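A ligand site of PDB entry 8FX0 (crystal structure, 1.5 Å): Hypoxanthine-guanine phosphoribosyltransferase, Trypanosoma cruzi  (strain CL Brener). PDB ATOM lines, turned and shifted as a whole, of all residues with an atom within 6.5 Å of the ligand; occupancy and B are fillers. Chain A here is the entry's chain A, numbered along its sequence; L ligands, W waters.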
ATOM      1  N   VAL A  83      24.041  17.955  14.214  1.00  0.00           N
ATOM      2  CA  VAL A  83      22.996  17.735  15.263  1.00  0.00           C
ATOM      3  C   VAL A  83      22.138  19.001  15.386  1.00  0.00           C
ATOM      4  O   VAL A  83      22.639  19.989  15.909  1.00  0.00           O
ATOM      5  CB  VAL A  83      23.637  17.324  16.596  1.00  0.00           C
ATOM      6  CG1 VAL A  83      22.590  17.080  17.685  1.00  0.00           C
ATOM      7  CG2 VAL A  83      24.533  16.082  16.427  1.00  0.00           C
ATOM      8  N   LEU A  84      20.887  18.952  14.937  1.00  0.00           N
ATOM      9  CA  LEU A  84      19.960  20.090  15.008  1.00  0.00           C
ATOM     10  C   LEU A  84      19.453  20.233  16.449  1.00  0.00           C
ATOM     11  O   LEU A  84      19.520  19.264  17.173  1.00  0.00           O
ATOM     12  CB  LEU A  84      18.804  19.861  14.026  1.00  0.00           C
ATOM     13  CG  LEU A  84      19.152  19.924  12.540  1.00  0.00           C
ATOM     14  CD1 LEU A  84      17.929  19.556  11.681  1.00  0.00           C
ATOM     15  CD2 LEU A  84      19.686  21.314  12.156  1.00  0.00           C
ATOM     16  N   GLY A  86      20.919  23.225  17.475  1.00  0.00           N
ATOM     17  CA  GLY A  86      22.044  24.059  17.963  1.00  0.00           C
ATOM     18  C   GLY A  86      23.221  24.163  17.019  1.00  0.00           C
ATOM     19  O   GLY A  86      23.931  25.151  17.116  1.00  0.00           O
ATOM     20  N   MET A 124      17.491   9.884  27.043  1.00  0.00           N
ATOM     21  CA  MET A 124      17.617  10.408  25.649  1.00  0.00           C
ATOM     22  C   MET A 124      16.636   9.726  24.672  1.00  0.00           C
ATOM     23  O   MET A 124      16.345   8.550  24.861  1.00  0.00           O
ATOM     24  CB  MET A 124      19.043  10.200  25.124  1.00  0.00           C
ATOM     25  CG  MET A 124      20.134  10.960  25.921  1.00  0.00           C
ATOM     26  SD  MET A 124      19.985  12.750  25.777  1.00  0.00           S
ATOM     27  CE  MET A 124      20.014  12.973  24.000  1.00  0.00           C
ATOM     28  N   GLU A 144      28.527  18.969  16.433  1.00  0.00           N
ATOM     29  CA  GLU A 144      27.626  19.223  17.588  1.00  0.00           C
ATOM     30  C   GLU A 144      27.975  20.612  18.160  1.00  0.00           C
ATOM     31  O   GLU A 144      29.060  21.064  17.969  1.00  0.00           O
ATOM     32  CB  GLU A 144      27.763  18.084  18.618  1.00  0.00           C
ATOM     33  CG  GLU A 144      27.013  18.257  19.944  1.00  0.00           C
ATOM     34  CD  GLU A 144      25.482  18.282  19.851  1.00  0.00           C
ATOM     35  OE1 GLU A 144      24.986  19.053  19.049  1.00  0.00           O
ATOM     36  OE2 GLU A 144      24.811  17.557  20.591  1.00  0.00           O
ATOM     37  N   ASP A 145      27.023  21.259  18.826  1.00  0.00           N
ATOM     38  CA  ASP A 145      27.220  22.637  19.355  1.00  0.00           C
ATOM     39  C   ASP A 145      28.124  22.591  20.594  1.00  0.00           C
ATOM     40  O   ASP A 145      29.072  23.359  20.657  1.00  0.00           O
ATOM     41  CB  ASP A 145      25.864  23.334  19.658  1.00  0.00           C
ATOM     42  CG  ASP A 145      24.951  22.601  20.607  1.00  0.00           C
ATOM     43  OD1 ASP A 145      25.323  21.508  20.974  1.00  0.00           O
ATOM     44  OD2 ASP A 145      23.900  23.136  20.963  1.00  0.00           O
ATOM     45  N   ILE A 146      27.813  21.741  21.566  1.00  0.00           N
ATOM     46  CA  ILE A 146      28.545  21.754  22.853  1.00  0.00           C
ATOM     47  C   ILE A 146      28.640  20.370  23.489  1.00  0.00           C
ATOM     48  O   ILE A 146      27.697  19.614  23.327  1.00  0.00           O
ATOM     49  CB  ILE A 146      27.908  22.775  23.838  1.00  0.00           C
ATOM     50  CG1 ILE A 146      28.783  23.003  25.084  1.00  0.00           C
ATOM     51  CG2 ILE A 146      26.485  22.387  24.239  1.00  0.00           C
ATOM     52  CD1 ILE A 146      28.449  24.306  25.851  1.00  0.00           C
ATOM     53  N   VAL A 147      29.764  20.063  24.127  1.00  0.00           N
ATOM     54  CA  VAL A 147      29.906  18.880  25.002  1.00  0.00           C
ATOM     55  C   VAL A 147      29.933  19.479  26.428  1.00  0.00           C
ATOM     56  O   VAL A 147      30.725  20.386  26.673  1.00  0.00           O
ATOM     57  CB  VAL A 147      31.143  17.997  24.702  1.00  0.00           C
ATOM     58  CG1 VAL A 147      32.477  18.754  24.779  1.00  0.00           C
ATOM     59  CG2 VAL A 147      31.172  16.769  25.627  1.00  0.00           C
ATOM     60  N   ASP A 148      29.039  19.031  27.292  1.00  0.00           N
ATOM     61  CA  ASP A 148      28.911  19.559  28.673  1.00  0.00           C
ATOM     62  C   ASP A 148      28.990  18.335  29.605  1.00  0.00           C
ATOM     63  O   ASP A 148      30.097  17.999  30.014  1.00  0.00           O
ATOM     64  CB  ASP A 148      27.652  20.448  28.710  1.00  0.00           C
ATOM     65  CG  ASP A 148      27.478  21.245  30.001  1.00  0.00           C
ATOM     66  OD1 ASP A 148      28.086  20.872  30.983  1.00  0.00           O
ATOM     67  OD2 ASP A 148      26.730  22.231  29.994  1.00  0.00           O
ATOM     68  N   SER A 149      27.875  17.682  29.925  1.00  0.00           N
ATOM     69  CA  SER A 149      27.874  16.427  30.736  1.00  0.00           C
ATOM     70  C   SER A 149      28.536  15.305  29.930  1.00  0.00           C
ATOM     71  O   SER A 149      29.076  14.406  30.536  1.00  0.00           O
ATOM     72  CB  SER A 149      26.473  16.005  31.196  1.00  0.00           C
ATOM     73  OG  SER A 149      25.646  15.627  30.106  1.00  0.00           O
ATOM     74  N   GLY A 150      28.426  15.333  28.604  1.00  0.00           N
ATOM     75  CA  GLY A 150      28.883  14.243  27.709  1.00  0.00           C
ATOM     76  C   GLY A 150      27.780  13.231  27.395  1.00  0.00           C
ATOM     77  O   GLY A 150      28.022  12.369  26.567  1.00  0.00           O
ATOM     78  N   LYS A 151      26.608  13.360  28.001  1.00  0.00           N
ATOM     79  CA  LYS A 151      25.539  12.330  27.848  1.00  0.00           C
ATOM     80  C   LYS A 151      24.922  12.334  26.447  1.00  0.00           C
ATOM     81  O   LYS A 151      24.681  11.262  25.900  1.00  0.00           O
ATOM     82  CB  LYS A 151      24.465  12.501  28.938  1.00  0.00           C
ATOM     83  CG  LYS A 151      24.977  12.263  30.361  1.00  0.00           C
ATOM     84  CD  LYS A 151      23.971  12.624  31.461  1.00  0.00           C
ATOM     85  CE  LYS A 151      24.534  12.479  32.870  1.00  0.00           C
ATOM     86  NZ  LYS A 151      24.862  11.056  33.216  1.00  0.00           N
ATOM     87  N   THR A 152      24.703  13.512  25.871  1.00  0.00           N
ATOM     88  CA  THR A 152      24.082  13.592  24.518  1.00  0.00           C
ATOM     89  C   THR A 152      25.004  12.883  23.493  1.00  0.00           C
ATOM     90  O   THR A 152      24.503  12.084  22.723  1.00  0.00           O
ATOM     91  CB  THR A 152      23.799  15.028  24.089  1.00  0.00           C
ATOM     92  OG1 THR A 152      22.888  15.570  25.045  1.00  0.00           O
ATOM     93  CG2 THR A 152      23.234  15.126  22.674  1.00  0.00           C
ATOM     94  N   LEU A 153      26.296  13.186  23.496  1.00  0.00           N
ATOM     95  CA  LEU A 153      27.217  12.624  22.484  1.00  0.00           C
ATOM     96  C   LEU A 153      27.457  11.121  22.737  1.00  0.00           C
ATOM     97  O   LEU A 153      27.587  10.411  21.784  1.00  0.00           O
ATOM     98  CB  LEU A 153      28.539  13.394  22.437  1.00  0.00           C
ATOM     99  CG  LEU A 153      28.525  14.719  21.653  1.00  0.00           C
ATOM    100  CD1 LEU A 153      29.791  15.529  21.958  1.00  0.00           C
ATOM    101  CD2 LEU A 153      28.382  14.459  20.144  1.00  0.00           C
ATOM    102  N   LYS A 177      32.707  22.582  27.355  1.00  0.00           N
ATOM    103  CA  LYS A 177      32.606  23.095  28.746  1.00  0.00           C
ATOM    104  C   LYS A 177      33.266  22.020  29.616  1.00  0.00           C
ATOM    105  O   LYS A 177      32.577  21.115  30.052  1.00  0.00           O
ATOM    106  CB  LYS A 177      31.148  23.368  29.115  1.00  0.00           C
ATOM    107  CG  LYS A 177      30.952  24.071  30.456  1.00  0.00           C
ATOM    108  CD  LYS A 177      29.472  24.170  30.882  1.00  0.00           C
ATOM    109  CE  LYS A 177      28.578  24.821  29.820  1.00  0.00           C
ATOM    110  NZ  LYS A 177      27.181  24.991  30.331  1.00  0.00           N
ATOM    111  N   VAL A 194      34.690  26.969  26.750  1.00  0.00           N
ATOM    112  CA  VAL A 194      33.791  27.947  27.395  1.00  0.00           C
ATOM    113  C   VAL A 194      33.855  27.764  28.917  1.00  0.00           C
ATOM    114  O   VAL A 194      34.211  26.688  29.372  1.00  0.00           O
ATOM    115  CB  VAL A 194      32.355  27.792  26.855  1.00  0.00           C
ATOM    116  CG1 VAL A 194      32.329  27.990  25.325  1.00  0.00           C
ATOM    117  CG2 VAL A 194      31.700  26.455  27.243  1.00  0.00           C
ATOM    118  N   LYS A 197      29.474  27.750  32.756  1.00  0.00           N
ATOM    119  CA  LYS A 197      28.260  28.585  32.916  1.00  0.00           C
ATOM    120  C   LYS A 197      27.385  28.296  31.691  1.00  0.00           C
ATOM    121  O   LYS A 197      27.903  27.775  30.727  1.00  0.00           O
ATOM    122  CB  LYS A 197      28.636  30.067  32.914  1.00  0.00           C
ATOM    123  CG  LYS A 197      29.504  30.548  34.081  1.00  0.00           C
ATOM    124  CD  LYS A 197      28.821  30.406  35.453  1.00  0.00           C
ATOM    125  CE  LYS A 197      29.671  30.925  36.615  1.00  0.00           C
ATOM    126  NZ  LYS A 197      29.567  32.416  36.786  1.00  0.00           N
ATOM    127  N   TYR A 198      26.118  28.658  31.761  1.00  0.00           N
ATOM    128  CA  TYR A 198      25.191  28.490  30.614  1.00  0.00           C
ATOM    129  C   TYR A 198      25.568  29.532  29.543  1.00  0.00           C
ATOM    130  O   TYR A 198      25.514  30.711  29.853  1.00  0.00           O
ATOM    131  CB  TYR A 198      23.734  28.645  31.056  1.00  0.00           C
ATOM    132  CG  TYR A 198      22.736  28.198  30.016  1.00  0.00           C
ATOM    133  CD1 TYR A 198      22.286  29.060  29.030  1.00  0.00           C
ATOM    134  CD2 TYR A 198      22.252  26.896  30.002  1.00  0.00           C
ATOM    135  CE1 TYR A 198      21.383  28.650  28.067  1.00  0.00           C
ATOM    136  CE2 TYR A 198      21.339  26.467  29.045  1.00  0.00           C
ATOM    137  CZ  TYR A 198      20.895  27.358  28.082  1.00  0.00           C
ATOM    138  OH  TYR A 198      19.999  26.927  27.149  1.00  0.00           O
ATOM    139  N   VAL A 199      25.885  29.097  28.332  1.00  0.00           N
ATOM    140  CA  VAL A 199      26.319  30.015  27.228  1.00  0.00           C
ATOM    141  C   VAL A 199      25.156  30.341  26.266  1.00  0.00           C
ATOM    142  O   VAL A 199      24.205  29.667  26.170  1.00  0.00           O
ATOM    143  CB  VAL A 199      27.583  29.486  26.508  1.00  0.00           C
ATOM    144  CG1 VAL A 199      28.798  29.492  27.449  1.00  0.00           C
ATOM    145  CG2 VAL A 199      27.409  28.109  25.854  1.00  0.00           C
ATOM    146  N   ILE A 200      25.157  31.498  25.660  1.00  0.00           N
ATOM    147  CA  ILE A 200      24.081  31.895  24.720  1.00  0.00           C
ATOM    148  C   ILE A 200      24.782  32.551  23.527  1.00  0.00           C
ATOM    149  O   ILE A 200      25.880  33.005  23.691  1.00  0.00           O
ATOM    150  CB  ILE A 200      23.040  32.825  25.370  1.00  0.00           C
ATOM    151  CG1 ILE A 200      23.709  34.000  26.091  1.00  0.00           C
ATOM    152  CG2 ILE A 200      22.092  32.038  26.300  1.00  0.00           C
ATOM    153  CD1 ILE A 200      22.808  35.245  26.247  1.00  0.00           C
ATOM    154  N   PHE A 204      23.460  29.026  20.448  1.00  0.00           N
ATOM    155  CA  PHE A 204      23.087  28.696  21.840  1.00  0.00           C
ATOM    156  C   PHE A 204      21.905  29.599  22.197  1.00  0.00           C
ATOM    157  O   PHE A 204      21.879  30.734  21.766  1.00  0.00           O
ATOM    158  CB  PHE A 204      24.260  28.837  22.813  1.00  0.00           C
ATOM    159  CG  PHE A 204      25.415  27.911  22.513  1.00  0.00           C
ATOM    160  CD1 PHE A 204      25.258  26.542  22.620  1.00  0.00           C
ATOM    161  CD2 PHE A 204      26.654  28.402  22.132  1.00  0.00           C
ATOM    162  CE1 PHE A 204      26.309  25.685  22.355  1.00  0.00           C
ATOM    163  CE2 PHE A 204      27.713  27.551  21.865  1.00  0.00           C
ATOM    164  CZ  PHE A 204      27.540  26.186  21.979  1.00  0.00           C
ATOM    165  N   GLU A 205      20.973  29.077  23.005  1.00  0.00           N
ATOM    166  CA  GLU A 205      19.738  29.851  23.226  1.00  0.00           C
ATOM    167  C   GLU A 205      19.030  29.621  24.549  1.00  0.00           C
ATOM    168  O   GLU A 205      19.451  28.756  25.263  1.00  0.00           O
ATOM    169  CB  GLU A 205      18.732  29.514  22.104  1.00  0.00           C
ATOM    170  CG  GLU A 205      18.583  28.025  21.782  1.00  0.00           C
ATOM    171  CD  GLU A 205      17.962  27.144  22.864  1.00  0.00           C
ATOM    172  OE1 GLU A 205      16.840  27.441  23.291  1.00  0.00           O
ATOM    173  OE2 GLU A 205      18.579  26.151  23.259  1.00  0.00           O
HETATM  174  C1  LIG L   1      23.856  19.339  25.975  1.00  0.00           C
HETATM  175  C2  LIG L   1      24.772  25.638  27.313  1.00  0.00           C
HETATM  176  C3  LIG L   1      24.323  24.209  27.381  1.00  0.00           C
HETATM  177  C4  LIG L   1      23.229  23.798  26.666  1.00  0.00           C
HETATM  178  C5  LIG L   1      23.064  22.446  26.937  1.00  0.00           C
HETATM  179  C6  LIG L   1      24.099  22.139  27.818  1.00  0.00           C
HETATM  180  C7  LIG L   1      21.974  21.511  26.384  1.00  0.00           C
HETATM  181  C8  LIG L   1      22.981  19.771  24.778  1.00  0.00           C
HETATM  182  C9  LIG L   1      24.968  18.364  25.621  1.00  0.00           C
HETATM  183  C10 LIG L   1      23.752  19.761  23.431  1.00  0.00           C
HETATM  184  C11 LIG L   1      22.956  26.164  25.787  1.00  0.00           C
HETATM  185  N1  LIG L   1      24.824  23.190  28.045  1.00  0.00           N
HETATM  186  N2  LIG L   1      22.251  21.025  25.024  1.00  0.00           N
HETATM  187  N3  LIG L   1      22.519  24.781  25.841  1.00  0.00           N
HETATM  188  N4  LIG L   1      24.101  26.578  26.531  1.00  0.00           N
HETATM  189  O1  LIG L   1      26.740  16.982  26.806  1.00  0.00           O
HETATM  190  O2  LIG L   1      24.536  16.270  27.232  1.00  0.00           O
HETATM  191  O3  LIG L   1      25.177  18.170  28.328  1.00  0.00           O
HETATM  192  O4  LIG L   1      22.968  20.450  22.482  1.00  0.00           O
HETATM  193  O5  LIG L   1      25.680  25.957  27.911  1.00  0.00           O
HETATM  194  P1  LIG L   1      25.425  17.405  27.114  1.00  0.00           P
HETATM  195  O   HOH W   1      21.326  26.174  23.260  1.00  0.00           O
HETATM  196  O   HOH W   2      19.510  24.215  26.146  1.00  0.00           O
HETATM  197  O   HOH W   3      22.414  15.815  28.611  1.00  0.00           O
HETATM  198  O   HOH W   4      22.221  23.164  23.428  1.00  0.00           O
HETATM  199  O   HOH W   5      22.004  18.149  20.913  1.00  0.00           O
HETATM  200  O   HOH W   6      26.249  17.236  22.969  1.00  0.00           O
HETATM  201  O   HOH W   7      23.628  19.301  30.023  1.00  0.00           O
HETATM  202  O   HOH W   8      27.523  15.596  24.739  1.00  0.00           O
HETATM  203  O   HOH W   9      19.800  19.603  24.819  1.00  0.00           O
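Water W8 bridges O1 of the ligand and N of Leu 153. Water W4 bridges a nitrogen (N2) of the ligand and the side-chain carboxylate of Asp 145. Water W5 bridges the side-chain carboxylate of Glu 144 (2.9 Å) and an oxygen (O4) of the ligand (2.9 Å). Water W1 bridges OE2 of Glu 205 (2.7 Å) and N3 of the ligand (3.2 Å). Water W2 bridges OH of Tyr 198 and N3 of the ligand. Water W6 bridges OE2 of Glu 144 and O of Ile 146.
OD2 of Asp 148 is in salt-bridge range of NZ of Lys 177 (2.8 Å). The side-chain amino group of Lys 177 sits at hydrogen-bond distance from the backbone carbonyl oxygen of Lys 197 (2.9 Å). The backbone NH (N) of Lys 177 sits at hydrogen-bond distance from the backbone carbonyl oxygen (O) of Val 147 (3.0 Å). The backbone NH (N) of Lys 151 is in hydrogen-bond range of the side-chain hydroxyl (OG) of Ser 149 (3.2 Å). The backbone carbonyl oxygen (O) of Glu 205 lies within hydrogen-bond range of the side-chain hydroxyl (OH) of Tyr 198 (2.7 Å).
OE2 of Glu 144 touches C10 of the ligand (3.7 Å). Ile 146 touches the ligand. N of Lys 151 touches O2 of the ligand, at 3.7 Å. Tyr 198 touches the ligand (CZ to C11, 3.3 Å). CD1 of Phe 204 touches C11 of the ligand, at 3.9 Å. Hydrophobic or aromatic side chains that line the ligand: Ile 146, Tyr 198, Val 199 and Phe 204. 12 residues have an atom within 4 Å of the ligand: Glu 144, Asp 145, Ile 146, Asp 148, Ser 149, Gly 150, Lys 151, Thr 152, Lys 177, Tyr 198, Val 199 and Phe 204. The nearest printed residue that does not touch the ligand is Lys 197 (4.02 Å).
N of Thr 152 lies within hydrogen-bond range of O2 of the ligand (3.1 Å). The side-chain hydroxyl (OG1) of Thr 152 lies within hydrogen-bond range of an oxygen (O2) of the ligand, 2.8 Å away. N of Asp 148 lies within hydrogen-bond range of O1 of the ligand (3.1 Å). N1 of the ligand is in hydrogen-bond range of OD2 of Asp 148. N of Gly 150 lies within hydrogen-bond range of O1 of the ligand, at 3.0 Å. The side-chain carboxylate of Asp 145 sits at hydrogen-bond distance from an oxygen (O4) of the ligand (3.0 Å). NZ of Lys 177 lies within hydrogen-bond range of O5 of the ligand, at 3.0 Å. An oxygen (O5) of the ligand lies within hydrogen-bond range of the backbone NH (N) of Val 199 (3.2 Å). O of Val 199 lies within hydrogen-bond range of N4 of the ligand, at 3.1 Å. The backbone NH (N) of Ser 149 lies within hydrogen-bond range of an oxygen (O3) of the ligand (3.2 Å). The side-chain hydroxyl of Ser 149 lies within hydrogen-bond range of an oxygen (O3) of the ligand.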
